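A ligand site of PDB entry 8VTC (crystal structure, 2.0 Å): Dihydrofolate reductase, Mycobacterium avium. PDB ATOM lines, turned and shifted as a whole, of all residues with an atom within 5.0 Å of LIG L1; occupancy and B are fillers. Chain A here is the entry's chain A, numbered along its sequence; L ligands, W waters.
A nitrogen (N2) of LIG L1 is in hydrogen-bond range of the guanidinium group of Arg 71 (3.3 Å).
An oxygen (O1) of LIG L1 is in hydrogen-bond range of the backbone NH of Ile 107, at 3.3 Å.
N of Ala 105 sits at hydrogen-bond distance from O8 of LIG L1 (3.1 Å).
The guanidinium group of Arg 49 lies within salt-bridge range of an oxygen (O9) of LIG L1, 3.5 Å away.
The guanidinium group (NH2) of Arg 48 is in salt-bridge range of an oxygen (O15) of LIG L1, at 2.7 Å.
N of Gln 106 lies within hydrogen-bond range of O8 of LIG L1 (3.0 Å).
The backbone carbonyl oxygen (O) of Gly 22 is in hydrogen-bond range of an oxygen (O13) of LIG L1, at 3.5 Å.
The backbone NH (N) of Arg 71 sits at hydrogen-bond distance from an oxygen (O17) of LIG L1 (2.7 Å).
N of Arg 49 lies within hydrogen-bond range of O3 of LIG L1.
The backbone carbonyl oxygen (O) of Ala 11 sits at hydrogen-bond distance from a nitrogen (N7) of LIG L1 (2.7 Å).
An oxygen (O2) of LIG L1 is in hydrogen-bond range of the backbone NH of Thr 50, at 3.1 Å.
O2 of LIG L1 is in hydrogen-bond range of OG1 of Thr 50 (2.7 Å).
O of Val 9 lies within hydrogen-bond range of N4 of LG2 L2 (2.8 Å).
OH of Tyr 108 is in hydrogen-bond range of N4 of LG2 L2, 3.5 Å away.
The guanidinium group (NH2) of Arg 72 lies within salt-bridge range of an oxygen (O16) of LIG L1.
OG of Ser 70 lies within hydrogen-bond range of O16 of LIG L1 (2.7 Å).
An oxygen (O13) of LIG L1 lies within hydrogen-bond range of the side-chain hydroxyl (OG) of Ser 53, 3.0 Å away.
A nitrogen (N4) of LG2 L2 sits at hydrogen-bond distance from the backbone carbonyl oxygen of Ile 102 (3.0 Å).
A nitrogen (N7) of LIG L1 lies within hydrogen-bond range of the backbone carbonyl oxygen of Ile 18 (3.1 Å).
The backbone NH (N) of Ala 11 is in hydrogen-bond range of an oxygen (O14) of LIG L1, 2.8 Å away.
O2 of LIG L1 lies within hydrogen-bond range of N of Gly 104 (2.9 Å).
OG of Ser 70 sits at hydrogen-bond distance from N of Arg 72, 3.0 Å away.
The backbone NH of Gly 104 sits at hydrogen-bond distance from the side-chain hydroxyl of Thr 50, at 2.9 Å.
The backbone NH (N) of Ile 18 sits at hydrogen-bond distance from the backbone carbonyl oxygen (O) of Ala 134.
The backbone carbonyl oxygen (O) of Val 9 sits at hydrogen-bond distance from the side-chain hydroxyl (OH) of Tyr 108, at 2.6 Å.
The backbone carbonyl oxygen of Gly 103 lies within hydrogen-bond range of the backbone NH of Gly 47, 2.8 Å away.
The guanidinium group of Arg 49 sits close to the side-chain amide nitrogen of Gln 106 (3.2 Å).
OG of Ser 53 is in hydrogen-bond range of O of Gly 22 (2.5 Å).
O of Gly 19 is in hydrogen-bond range of N of Ala 134, 2.9 Å away.
Trp 10 touches LIG L1 (CA to O14, 3.4 Å).
Gly 19 touches LIG L1.
Asp 23 touches LIG L1.
Ile 24 touches LIG L1.
CZ2 of Trp 26 touches N7 of LIG L1, 3.97 Å away.
CA of Gly 47 touches O3 of LIG L1 (3.5 Å).
Val 69 touches LIG L1.
Gly 84 touches LIG L1.
Ile 102 touches LIG L1 (O to C20, 3.2 Å).
CA of Gly 103 touches C20 of LIG L1 (3.9 Å).
OH of Tyr 108 touches C19 of LIG L1, 3.7 Å away.
CD1 of Leu 110 touches N3 of LIG L1 (3.5 Å).
CB of Ala 134 touches O11 of LIG L1, 3.8 Å away.
Hydrophobic or aromatic side chains that line LIG L1: Trp 10, Ala 11, Ile 18, Ile 24, Trp 26, Val 69, Ala 105, Ile 107, Leu 110 and Ala 134.
Within 4 Å of LIG L1: Trp 10, Ala 11, Ile 18, Gly 19, Gly 22, Asp 23, Ile 24, Trp 26, Gly 47, Arg 48, Arg 49, Thr 50, Ser 53, Val 69, Ser 70, Arg 71, Arg 72, Gly 84, Ile 102, Gly 103, Gly 104, Ala 105, Gln 106, Ile 107, Tyr 108, Leu 110 and Ala 134.
Water W2 lies within hydrogen-bond range of N4 of LIG L1 and O of Gly 84.
Water W1 lies within hydrogen-bond range of the guanidinium group (NH1) of Arg 71 (2.5 Å) and an oxygen (O17) of LIG L1 (2.7 Å).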
ATOM      1  N   VAL A   9     -12.243  12.405  10.489  1.00  0.00           N
ATOM      2  CA  VAL A   9     -11.205  12.119  11.468  1.00  0.00           C
ATOM      3  C   VAL A   9     -10.784  13.419  12.161  1.00  0.00           C
ATOM      4  O   VAL A   9     -10.517  14.429  11.506  1.00  0.00           O
ATOM      5  CB  VAL A   9     -10.037  11.378  10.813  1.00  0.00           C
ATOM      6  CG1 VAL A   9      -9.428  12.195   9.681  1.00  0.00           C
ATOM      7  CG2 VAL A   9      -8.972  10.979  11.828  1.00  0.00           C
ATOM      8  N   TRP A  10     -10.708  13.372  13.514  1.00  0.00           N
ATOM      9  CA  TRP A  10     -10.253  14.517  14.293  1.00  0.00           C
ATOM     10  C   TRP A  10      -9.722  14.093  15.664  1.00  0.00           C
ATOM     11  O   TRP A  10      -9.931  12.958  16.099  1.00  0.00           O
ATOM     12  CB  TRP A  10     -11.366  15.554  14.499  1.00  0.00           C
ATOM     13  CG  TRP A  10     -12.459  15.227  15.488  1.00  0.00           C
ATOM     14  CD1 TRP A  10     -12.492  15.484  16.824  1.00  0.00           C
ATOM     15  CD2 TRP A  10     -13.731  14.623  15.172  1.00  0.00           C
ATOM     16  NE1 TRP A  10     -13.693  15.095  17.361  1.00  0.00           N
ATOM     17  CE2 TRP A  10     -14.478  14.570  16.362  1.00  0.00           C
ATOM     18  CE3 TRP A  10     -14.319  14.134  13.995  1.00  0.00           C
ATOM     19  CZ2 TRP A  10     -15.753  14.035  16.420  1.00  0.00           C
ATOM     20  CZ3 TRP A  10     -15.591  13.590  14.058  1.00  0.00           C
ATOM     21  CH2 TRP A  10     -16.309  13.566  15.240  1.00  0.00           C
ATOM     22  N   ALA A  11      -9.069  15.074  16.308  1.00  0.00           N
ATOM     23  CA  ALA A  11      -8.597  15.000  17.672  1.00  0.00           C
ATOM     24  C   ALA A  11      -9.224  16.152  18.440  1.00  0.00           C
ATOM     25  O   ALA A  11      -9.204  17.302  17.975  1.00  0.00           O
ATOM     26  CB  ALA A  11      -7.073  15.066  17.747  1.00  0.00           C
ATOM     27  N   GLN A  12      -9.742  15.821  19.620  1.00  0.00           N
ATOM     28  CA  GLN A  12     -10.346  16.787  20.514  1.00  0.00           C
ATOM     29  C   GLN A  12      -9.880  16.563  21.955  1.00  0.00           C
ATOM     30  O   GLN A  12      -9.613  15.443  22.383  1.00  0.00           O
ATOM     31  CB  GLN A  12     -11.870  16.720  20.439  1.00  0.00           C
ATOM     32  CG  GLN A  12     -12.462  15.393  20.885  1.00  0.00           C
ATOM     33  CD  GLN A  12     -13.972  15.456  21.016  1.00  0.00           C
ATOM     34  OE1 GLN A  12     -14.721  15.139  20.082  1.00  0.00           O
ATOM     35  NE2 GLN A  12     -14.425  15.889  22.189  1.00  0.00           N
ATOM     36  N   ILE A  18     -10.858  21.501  19.275  1.00  0.00           N
ATOM     37  CA  ILE A  18      -9.957  20.931  18.278  1.00  0.00           C
ATOM     38  C   ILE A  18      -8.930  21.966  17.843  1.00  0.00           C
ATOM     39  O   ILE A  18      -7.885  21.572  17.334  1.00  0.00           O
ATOM     40  CB  ILE A  18     -10.719  20.355  17.066  1.00  0.00           C
ATOM     41  CG1 ILE A  18     -11.400  21.443  16.218  1.00  0.00           C
ATOM     42  CG2 ILE A  18     -11.725  19.300  17.516  1.00  0.00           C
ATOM     43  CD1 ILE A  18     -11.970  20.950  14.905  1.00  0.00           C
ATOM     44  N   GLY A  19      -9.215  23.269  17.982  1.00  0.00           N
ATOM     45  CA  GLY A  19      -8.300  24.283  17.488  1.00  0.00           C
ATOM     46  C   GLY A  19      -8.385  25.553  18.318  1.00  0.00           C
ATOM     47  O   GLY A  19      -9.456  25.940  18.780  1.00  0.00           O
ATOM     48  N   ARG A  20      -7.235  26.217  18.461  1.00  0.00           N
ATOM     49  CA  ARG A  20      -7.177  27.492  19.135  1.00  0.00           C
ATOM     50  C   ARG A  20      -6.038  28.315  18.550  1.00  0.00           C
ATOM     51  O   ARG A  20      -4.910  27.825  18.429  1.00  0.00           O
ATOM     52  CB  ARG A  20      -6.984  27.280  20.642  1.00  0.00           C
ATOM     53  CG  ARG A  20      -6.830  28.547  21.469  1.00  0.00           C
ATOM     54  CD  ARG A  20      -6.820  28.271  22.970  1.00  0.00           C
ATOM     55  NE  ARG A  20      -8.106  27.762  23.487  1.00  0.00           N
ATOM     56  CZ  ARG A  20      -8.278  27.281  24.720  1.00  0.00           C
ATOM     57  NH1 ARG A  20      -7.265  27.239  25.575  1.00  0.00           N
ATOM     58  NH2 ARG A  20      -9.467  26.846  25.111  1.00  0.00           N
ATOM     59  N   GLY A  22      -5.498  29.121  15.616  1.00  0.00           N
ATOM     60  CA  GLY A  22      -5.128  28.631  14.288  1.00  0.00           C
ATOM     61  C   GLY A  22      -4.288  27.357  14.329  1.00  0.00           C
ATOM     62  O   GLY A  22      -3.837  26.863  13.290  1.00  0.00           O
ATOM     63  N   ASP A  23      -4.105  26.805  15.533  1.00  0.00           N
ATOM     64  CA  ASP A  23      -3.276  25.627  15.750  1.00  0.00           C
ATOM     65  C   ASP A  23      -4.076  24.574  16.511  1.00  0.00           C
ATOM     66  O   ASP A  23      -5.137  24.857  17.063  1.00  0.00           O
ATOM     67  CB  ASP A  23      -2.055  25.960  16.587  1.00  0.00           C
ATOM     68  CG  ASP A  23      -1.040  26.882  15.934  1.00  0.00           C
ATOM     69  OD1 ASP A  23      -1.178  27.151  14.739  1.00  0.00           O
ATOM     70  OD2 ASP A  23      -0.127  27.352  16.642  1.00  0.00           O
ATOM     71  N   ILE A  24      -3.471  23.392  16.611  1.00  0.00           N
ATOM     72  CA  ILE A  24      -3.921  22.360  17.532  1.00  0.00           C
ATOM     73  C   ILE A  24      -3.241  22.611  18.871  1.00  0.00           C
ATOM     74  O   ILE A  24      -2.031  22.724  18.920  1.00  0.00           O
ATOM     75  CB  ILE A  24      -3.598  20.967  16.976  1.00  0.00           C
ATOM     76  CG1 ILE A  24      -4.268  20.782  15.599  1.00  0.00           C
ATOM     77  CG2 ILE A  24      -3.990  19.899  17.996  1.00  0.00           C
ATOM     78  CD1 ILE A  24      -4.164  19.398  15.019  1.00  0.00           C
ATOM     79  N   TRP A  26      -2.131  21.258  21.547  1.00  0.00           N
ATOM     80  CA  TRP A  26      -1.395  20.256  22.296  1.00  0.00           C
ATOM     81  C   TRP A  26      -0.398  19.650  21.325  1.00  0.00           C
ATOM     82  O   TRP A  26      -0.450  19.894  20.117  1.00  0.00           O
ATOM     83  CB  TRP A  26      -2.317  19.177  22.876  1.00  0.00           C
ATOM     84  CG  TRP A  26      -3.165  18.527  21.810  1.00  0.00           C
ATOM     85  CD1 TRP A  26      -2.748  17.644  20.878  1.00  0.00           C
ATOM     86  CD2 TRP A  26      -4.568  18.759  21.551  1.00  0.00           C
ATOM     87  NE1 TRP A  26      -3.793  17.276  20.065  1.00  0.00           N
ATOM     88  CE2 TRP A  26      -4.914  17.956  20.448  1.00  0.00           C
ATOM     89  CE3 TRP A  26      -5.551  19.561  22.135  1.00  0.00           C
ATOM     90  CZ2 TRP A  26      -6.200  17.953  19.920  1.00  0.00           C
ATOM     91  CZ3 TRP A  26      -6.814  19.569  21.589  1.00  0.00           C
ATOM     92  CH2 TRP A  26      -7.133  18.764  20.512  1.00  0.00           C
ATOM     93  N   GLY A  47     -11.216  22.139   5.027  1.00  0.00           N
ATOM     94  CA  GLY A  47     -11.554  23.544   4.915  1.00  0.00           C
ATOM     95  C   GLY A  47     -10.332  24.406   4.588  1.00  0.00           C
ATOM     96  O   GLY A  47      -9.189  24.013   4.813  1.00  0.00           O
ATOM     97  N   ARG A  48     -10.587  25.576   4.042  1.00  0.00           N
ATOM     98  CA  ARG A  48      -9.493  26.447   3.630  1.00  0.00           C
ATOM     99  C   ARG A  48      -8.594  26.813   4.820  1.00  0.00           C
ATOM    100  O   ARG A  48      -7.364  26.892   4.672  1.00  0.00           O
ATOM    101  CB  ARG A  48     -10.092  27.587   2.810  1.00  0.00           C
ATOM    102  CG  ARG A  48      -9.050  28.498   2.163  1.00  0.00           C
ATOM    103  CD  ARG A  48      -8.560  29.581   3.123  1.00  0.00           C
ATOM    104  NE  ARG A  48      -9.688  30.465   3.452  1.00  0.00           N
ATOM    105  CZ  ARG A  48      -9.674  31.410   4.383  1.00  0.00           C
ATOM    106  NH1 ARG A  48      -8.619  31.571   5.172  1.00  0.00           N
ATOM    107  NH2 ARG A  48     -10.738  32.188   4.527  1.00  0.00           N
ATOM    108  N   ARG A  49      -9.142  27.045   6.006  1.00  0.00           N
ATOM    109  CA  ARG A  49      -8.288  27.490   7.101  1.00  0.00           C
ATOM    110  C   ARG A  49      -7.399  26.365   7.619  1.00  0.00           C
ATOM    111  O   ARG A  49      -6.298  26.638   8.087  1.00  0.00           O
ATOM    112  CB  ARG A  49      -9.054  28.002   8.316  1.00  0.00           C
ATOM    113  CG  ARG A  49      -9.854  29.217   7.967  1.00  0.00           C
ATOM    114  CD  ARG A  49     -10.317  29.762   9.279  1.00  0.00           C
ATOM    115  NE  ARG A  49     -11.175  30.873   8.899  1.00  0.00           N
ATOM    116  CZ  ARG A  49     -12.450  31.002   9.193  1.00  0.00           C
ATOM    117  NH1 ARG A  49     -12.955  30.435  10.289  1.00  0.00           N
ATOM    118  NH2 ARG A  49     -13.202  31.782   8.430  1.00  0.00           N
ATOM    119  N   THR A  50      -7.910  25.124   7.598  1.00  0.00           N
ATOM    120  CA  THR A  50      -7.094  23.989   8.003  1.00  0.00           C
ATOM    121  C   THR A  50      -5.874  23.874   7.074  1.00  0.00           C
ATOM    122  O   THR A  50      -4.750  23.623   7.528  1.00  0.00           O
ATOM    123  CB  THR A  50      -7.923  22.703   7.941  1.00  0.00           C
ATOM    124  OG1 THR A  50      -8.841  22.695   9.032  1.00  0.00           O
ATOM    125  CG2 THR A  50      -7.066  21.464   8.015  1.00  0.00           C
ATOM    126  N   SER A  53      -3.473  26.225   8.272  1.00  0.00           N
ATOM    127  CA  SER A  53      -2.922  25.799   9.555  1.00  0.00           C
ATOM    128  C   SER A  53      -1.727  24.864   9.383  1.00  0.00           C
ATOM    129  O   SER A  53      -0.806  24.868  10.202  1.00  0.00           O
ATOM    130  CB  SER A  53      -3.974  25.110  10.373  1.00  0.00           C
ATOM    131  OG  SER A  53      -3.506  24.936  11.700  1.00  0.00           O
ATOM    132  N   VAL A  69     -11.643  23.066   0.520  1.00  0.00           N
ATOM    133  CA  VAL A  69     -12.980  23.588   0.309  1.00  0.00           C
ATOM    134  C   VAL A  69     -12.936  25.067   0.606  1.00  0.00           C
ATOM    135  O   VAL A  69     -12.558  25.460   1.705  1.00  0.00           O
ATOM    136  CB  VAL A  69     -14.005  22.858   1.192  1.00  0.00           C
ATOM    137  CG1 VAL A  69     -15.396  23.446   1.056  1.00  0.00           C
ATOM    138  CG2 VAL A  69     -14.027  21.347   0.932  1.00  0.00           C
ATOM    139  N   SER A  70     -13.336  25.862  -0.387  1.00  0.00           N
ATOM    140  CA  SER A  70     -13.358  27.323  -0.293  1.00  0.00           C
ATOM    141  C   SER A  70     -14.603  27.827  -1.023  1.00  0.00           C
ATOM    142  O   SER A  70     -15.016  27.177  -1.985  1.00  0.00           O
ATOM    143  CB  SER A  70     -12.137  27.944  -0.916  1.00  0.00           C
ATOM    144  OG  SER A  70     -12.214  29.358  -0.762  1.00  0.00           O
ATOM    145  N   ARG A  71     -15.115  28.996  -0.626  1.00  0.00           N
ATOM    146  CA  ARG A  71     -16.177  29.653  -1.383  1.00  0.00           C
ATOM    147  C   ARG A  71     -15.597  30.337  -2.622  1.00  0.00           C
ATOM    148  O   ARG A  71     -16.325  30.623  -3.577  1.00  0.00           O
ATOM    149  CB  ARG A  71     -16.960  30.622  -0.503  1.00  0.00           C
ATOM    150  CG  ARG A  71     -17.757  29.887   0.567  1.00  0.00           C
ATOM    151  CD  ARG A  71     -19.012  30.607   0.979  1.00  0.00           C
ATOM    152  NE  ARG A  71     -19.688  29.799   2.010  1.00  0.00           N
ATOM    153  CZ  ARG A  71     -19.336  29.770   3.287  1.00  0.00           C
ATOM    154  NH1 ARG A  71     -18.308  30.486   3.732  1.00  0.00           N
ATOM    155  NH2 ARG A  71     -20.018  29.053   4.129  1.00  0.00           N
ATOM    156  N   ARG A  72     -14.279  30.606  -2.589  1.00  0.00           N
ATOM    157  CA  ARG A  72     -13.619  31.391  -3.609  1.00  0.00           C
ATOM    158  C   ARG A  72     -13.161  30.480  -4.740  1.00  0.00           C
ATOM    159  O   ARG A  72     -12.195  29.728  -4.602  1.00  0.00           O
ATOM    160  CB  ARG A  72     -12.353  32.057  -3.070  1.00  0.00           C
ATOM    161  CG  ARG A  72     -12.715  33.179  -2.117  1.00  0.00           C
ATOM    162  CD  ARG A  72     -11.432  33.820  -1.569  1.00  0.00           C
ATOM    163  NE  ARG A  72     -11.080  33.304  -0.241  1.00  0.00           N
ATOM    164  CZ  ARG A  72      -9.931  33.485   0.408  1.00  0.00           C
ATOM    165  NH1 ARG A  72      -8.826  33.854  -0.223  1.00  0.00           N
ATOM    166  NH2 ARG A  72      -9.901  33.265   1.703  1.00  0.00           N
ATOM    167  N   GLY A  84     -15.616  24.066  -4.372  1.00  0.00           N
ATOM    168  CA  GLY A  84     -16.486  25.140  -3.949  1.00  0.00           C
ATOM    169  C   GLY A  84     -17.590  24.653  -3.018  1.00  0.00           C
ATOM    170  O   GLY A  84     -18.480  25.405  -2.644  1.00  0.00           O
ATOM    171  N   SER A  85     -17.549  23.373  -2.642  1.00  0.00           N
ATOM    172  CA  SER A  85     -18.529  22.819  -1.742  1.00  0.00           C
ATOM    173  C   SER A  85     -18.067  21.446  -1.297  1.00  0.00           C
ATOM    174  O   SER A  85     -17.176  20.834  -1.882  1.00  0.00           O
ATOM    175  CB  SER A  85     -19.920  22.709  -2.366  1.00  0.00           C
ATOM    176  OG  SER A  85     -19.961  21.666  -3.336  1.00  0.00           O
ATOM    177  N   ILE A 102     -10.839  15.888   7.061  1.00  0.00           N
ATOM    178  CA  ILE A 102      -9.756  16.026   8.021  1.00  0.00           C
ATOM    179  C   ILE A 102      -9.786  17.395   8.731  1.00  0.00           C
ATOM    180  O   ILE A 102      -8.828  17.759   9.407  1.00  0.00           O
ATOM    181  CB  ILE A 102      -8.385  15.764   7.348  1.00  0.00           C
ATOM    182  CG1 ILE A 102      -7.947  16.869   6.372  1.00  0.00           C
ATOM    183  CG2 ILE A 102      -8.380  14.381   6.674  1.00  0.00           C
ATOM    184  CD1 ILE A 102      -6.461  16.859   6.060  1.00  0.00           C
ATOM    185  N   GLY A 103     -10.889  18.126   8.573  1.00  0.00           N
ATOM    186  CA  GLY A 103     -11.126  19.341   9.347  1.00  0.00           C
ATOM    187  C   GLY A 103     -11.277  20.574   8.458  1.00  0.00           C
ATOM    188  O   GLY A 103     -11.071  20.484   7.248  1.00  0.00           O
ATOM    189  N   GLY A 104     -11.630  21.736   9.039  1.00  0.00           N
ATOM    190  CA  GLY A 104     -11.765  21.962  10.475  1.00  0.00           C
ATOM    191  C   GLY A 104     -13.228  21.935  10.930  1.00  0.00           C
ATOM    192  O   GLY A 104     -14.020  21.168  10.411  1.00  0.00           O
ATOM    193  N   ALA A 105     -13.549  22.727  11.965  1.00  0.00           N
ATOM    194  CA  ALA A 105     -14.875  22.712  12.565  1.00  0.00           C
ATOM    195  C   ALA A 105     -15.978  22.959  11.527  1.00  0.00           C
ATOM    196  O   ALA A 105     -16.977  22.244  11.485  1.00  0.00           O
ATOM    197  CB  ALA A 105     -14.947  23.744  13.704  1.00  0.00           C
ATOM    198  N   GLN A 106     -15.823  23.971  10.693  1.00  0.00           N
ATOM    199  CA  GLN A 106     -16.872  24.289   9.738  1.00  0.00           C
ATOM    200  C   GLN A 106     -17.111  23.135   8.749  1.00  0.00           C
ATOM    201  O   GLN A 106     -18.251  22.794   8.450  1.00  0.00           O
ATOM    202  CB  GLN A 106     -16.539  25.565   8.963  1.00  0.00           C
ATOM    203  CG  GLN A 106     -16.452  26.818   9.833  1.00  0.00           C
ATOM    204  CD  GLN A 106     -16.282  28.061   9.007  1.00  0.00           C
ATOM    205  OE1 GLN A 106     -16.625  28.098   7.811  1.00  0.00           O
ATOM    206  NE2 GLN A 106     -15.761  29.102   9.626  1.00  0.00           N
ATOM    207  N   ILE A 107     -16.018  22.534   8.262  1.00  0.00           N
ATOM    208  CA  ILE A 107     -16.134  21.484   7.258  1.00  0.00           C
ATOM    209  C   ILE A 107     -16.719  20.170   7.821  1.00  0.00           C
ATOM    210  O   ILE A 107     -17.438  19.460   7.108  1.00  0.00           O
ATOM    211  CB  ILE A 107     -14.789  21.298   6.547  1.00  0.00           C
ATOM    212  CG1 ILE A 107     -14.729  22.108   5.229  1.00  0.00           C
ATOM    213  CG2 ILE A 107     -14.514  19.831   6.248  1.00  0.00           C
ATOM    214  CD1 ILE A 107     -15.276  23.522   5.298  1.00  0.00           C
ATOM    215  N   TYR A 108     -16.444  19.857   9.093  1.00  0.00           N
ATOM    216  CA  TYR A 108     -17.016  18.669   9.735  1.00  0.00           C
ATOM    217  C   TYR A 108     -18.542  18.781   9.738  1.00  0.00           C
ATOM    218  O   TYR A 108     -19.244  17.806   9.442  1.00  0.00           O
ATOM    219  CB  TYR A 108     -16.474  18.482  11.151  1.00  0.00           C
ATOM    220  CG  TYR A 108     -15.008  18.075  11.298  1.00  0.00           C
ATOM    221  CD1 TYR A 108     -14.473  17.025  10.561  1.00  0.00           C
ATOM    222  CD2 TYR A 108     -14.169  18.736  12.204  1.00  0.00           C
ATOM    223  CE1 TYR A 108     -13.136  16.670  10.687  1.00  0.00           C
ATOM    224  CE2 TYR A 108     -12.831  18.368  12.351  1.00  0.00           C
ATOM    225  CZ  TYR A 108     -12.315  17.342  11.582  1.00  0.00           C
ATOM    226  OH  TYR A 108     -10.999  16.984  11.669  1.00  0.00           O
ATOM    227  N   LEU A 110     -20.344  20.451   7.625  1.00  0.00           N
ATOM    228  CA  LEU A 110     -20.795  20.271   6.251  1.00  0.00           C
ATOM    229  C   LEU A 110     -20.848  18.797   5.877  1.00  0.00           C
ATOM    230  O   LEU A 110     -21.715  18.396   5.112  1.00  0.00           O
ATOM    231  CB  LEU A 110     -19.898  20.998   5.239  1.00  0.00           C
ATOM    232  CG  LEU A 110     -19.982  22.513   5.225  1.00  0.00           C
ATOM    233  CD1 LEU A 110     -18.967  23.052   4.199  1.00  0.00           C
ATOM    234  CD2 LEU A 110     -21.395  22.971   4.912  1.00  0.00           C
ATOM    235  N   ALA A 134     -12.101  26.490  17.861  1.00  0.00           N
ATOM    236  CA  ALA A 134     -12.693  25.557  16.919  1.00  0.00           C
ATOM    237  C   ALA A 134     -13.130  24.328  17.716  1.00  0.00           C
ATOM    238  O   ALA A 134     -12.327  23.757  18.469  1.00  0.00           O
ATOM    239  CB  ALA A 134     -11.671  25.228  15.855  1.00  0.00           C
HETATM  240  P1  LIG L   1     -12.114  25.157   8.440  1.00  0.00           P
HETATM  241  O1  LIG L   1     -13.339  24.369   8.707  1.00  0.00           O
HETATM  242  O2  LIG L   1     -10.807  24.457   8.289  1.00  0.00           O
HETATM  243  O3  LIG L   1     -12.275  26.081   7.148  1.00  0.00           O
HETATM  244  C1  LIG L   1     -13.305  27.073   7.066  1.00  0.00           C
HETATM  245  C2  LIG L   1     -13.298  27.601   5.663  1.00  0.00           C
HETATM  246  O4  LIG L   1     -13.900  26.624   4.781  1.00  0.00           O
HETATM  247  C3  LIG L   1     -14.075  28.894   5.408  1.00  0.00           C
HETATM  248  O5  LIG L   1     -13.291  30.005   5.806  1.00  0.00           O
HETATM  249  C4  LIG L   1     -14.237  28.803   3.904  1.00  0.00           C
HETATM  250  O6  LIG L   1     -13.035  29.118   3.194  1.00  0.00           O
HETATM  251  C5  LIG L   1     -14.519  27.309   3.713  1.00  0.00           C
HETATM  252  N1  LIG L   1     -15.927  26.991   3.759  1.00  0.00           N
HETATM  253  C6  LIG L   1     -16.731  26.863   4.859  1.00  0.00           C
HETATM  254  N2  LIG L   1     -17.969  26.541   4.572  1.00  0.00           N
HETATM  255  C7  LIG L   1     -17.964  26.459   3.186  1.00  0.00           C
HETATM  256  C8  LIG L   1     -18.969  26.145   2.265  1.00  0.00           C
HETATM  257  N3  LIG L   1     -20.222  25.856   2.617  1.00  0.00           N
HETATM  258  N4  LIG L   1     -18.626  26.134   0.958  1.00  0.00           N
HETATM  259  C9  LIG L   1     -17.359  26.405   0.610  1.00  0.00           C
HETATM  260  N5  LIG L   1     -16.329  26.703   1.386  1.00  0.00           N
HETATM  261  C10 LIG L   1     -16.707  26.715   2.671  1.00  0.00           C
HETATM  262  O7  LIG L   1     -11.983  26.256   9.601  1.00  0.00           O
HETATM  263  P2  LIG L   1     -12.172  26.209  11.180  1.00  0.00           P
HETATM  264  O8  LIG L   1     -13.586  25.819  11.435  1.00  0.00           O
HETATM  265  O9  LIG L   1     -11.682  27.522  11.687  1.00  0.00           O
HETATM  266  O10 LIG L   1     -11.191  25.056  11.696  1.00  0.00           O
HETATM  267  C11 LIG L   1      -9.738  25.290  11.617  1.00  0.00           C
HETATM  268  C12 LIG L   1      -9.112  25.067  12.975  1.00  0.00           C
HETATM  269  O11 LIG L   1      -9.251  23.668  13.301  1.00  0.00           O
HETATM  270  C13 LIG L   1      -7.619  25.381  13.123  1.00  0.00           C
HETATM  271  O12 LIG L   1      -7.322  25.878  14.416  1.00  0.00           O
HETATM  272  C14 LIG L   1      -6.973  24.006  12.925  1.00  0.00           C
HETATM  273  O13 LIG L   1      -5.669  23.945  13.499  1.00  0.00           O
HETATM  274  C15 LIG L   1      -7.991  23.113  13.639  1.00  0.00           C
HETATM  275  N6  LIG L   1      -7.954  21.672  13.223  1.00  0.00           N
HETATM  276  C16 LIG L   1      -7.820  20.706  14.192  1.00  0.00           C
HETATM  277  C17 LIG L   1      -7.917  19.372  13.917  1.00  0.00           C
HETATM  278  C18 LIG L   1      -7.935  18.377  15.022  1.00  0.00           C
HETATM  279  O14 LIG L   1      -8.246  17.222  14.711  1.00  0.00           O
HETATM  280  N7  LIG L   1      -7.595  18.692  16.272  1.00  0.00           N
HETATM  281  C19 LIG L   1      -7.988  18.924  12.500  1.00  0.00           C
HETATM  282  C20 LIG L   1      -7.990  20.029  11.514  1.00  0.00           C
HETATM  283  C21 LIG L   1      -8.013  21.295  11.896  1.00  0.00           C
HETATM  284  P3  LIG L   1     -13.083  30.505   2.383  1.00  0.00           P
HETATM  285  O15 LIG L   1     -13.154  31.540   3.481  1.00  0.00           O
HETATM  286  O16 LIG L   1     -11.761  30.536   1.631  1.00  0.00           O
HETATM  287  O17 LIG L   1     -14.281  30.494   1.476  1.00  0.00           O
HETATM  288  C1  LG2 L   2      -4.929  15.433  12.948  1.00  0.00           C
HETATM  289  N1  LG2 L   2      -5.253  14.519  13.882  1.00  0.00           N
HETATM  290  C2  LG2 L   2      -6.442  13.885  13.753  1.00  0.00           C
HETATM  291  N2  LG2 L   2      -6.733  12.922  14.637  1.00  0.00           N
HETATM  292  N3  LG2 L   2      -7.352  14.155  12.797  1.00  0.00           N
HETATM  293  C3  LG2 L   2      -7.032  15.111  11.903  1.00  0.00           C
HETATM  294  N4  LG2 L   2      -7.961  15.400  10.997  1.00  0.00           N
HETATM  295  C4  LG2 L   2      -5.782  15.791  11.918  1.00  0.00           C
HETATM  296  C5  LG2 L   2      -5.422  16.828  10.857  1.00  0.00           C
HETATM  297  C6  LG2 L   2      -4.085  17.538  10.991  1.00  0.00           C
HETATM  298  C7  LG2 L   2      -2.892  16.881  10.699  1.00  0.00           C
HETATM  299  C8  LG2 L   2      -1.675  17.554  10.841  1.00  0.00           C
HETATM  300  O1  LG2 L   2      -0.433  17.036  10.654  1.00  0.00           O
HETATM  301  C9  LG2 L   2      -0.326  15.713  10.149  1.00  0.00           C
HETATM  302  C10 LG2 L   2      -1.637  18.836  11.377  1.00  0.00           C
HETATM  303  O2  LG2 L   2      -0.402  19.427  11.459  1.00  0.00           O
HETATM  304  C11 LG2 L   2      -0.050  19.867  12.763  1.00  0.00           C
HETATM  305  C12 LG2 L   2      -2.838  19.521  11.614  1.00  0.00           C
HETATM  306  O3  LG2 L   2      -2.716  20.806  12.053  1.00  0.00           O
HETATM  307  C13 LG2 L   2      -3.878  21.612  12.085  1.00  0.00           C
HETATM  308  C14 LG2 L   2      -4.042  18.856  11.435  1.00  0.00           C
HETATM  309  O   HOH W   1     -16.372  31.753   2.689  1.00  0.00           O
HETATM  310  O   HOH W   2     -20.796  26.003  -0.665  1.00  0.00           O
HETATM  311  O   HOH W   3     -15.096  27.018  13.240  1.00  0.00           O
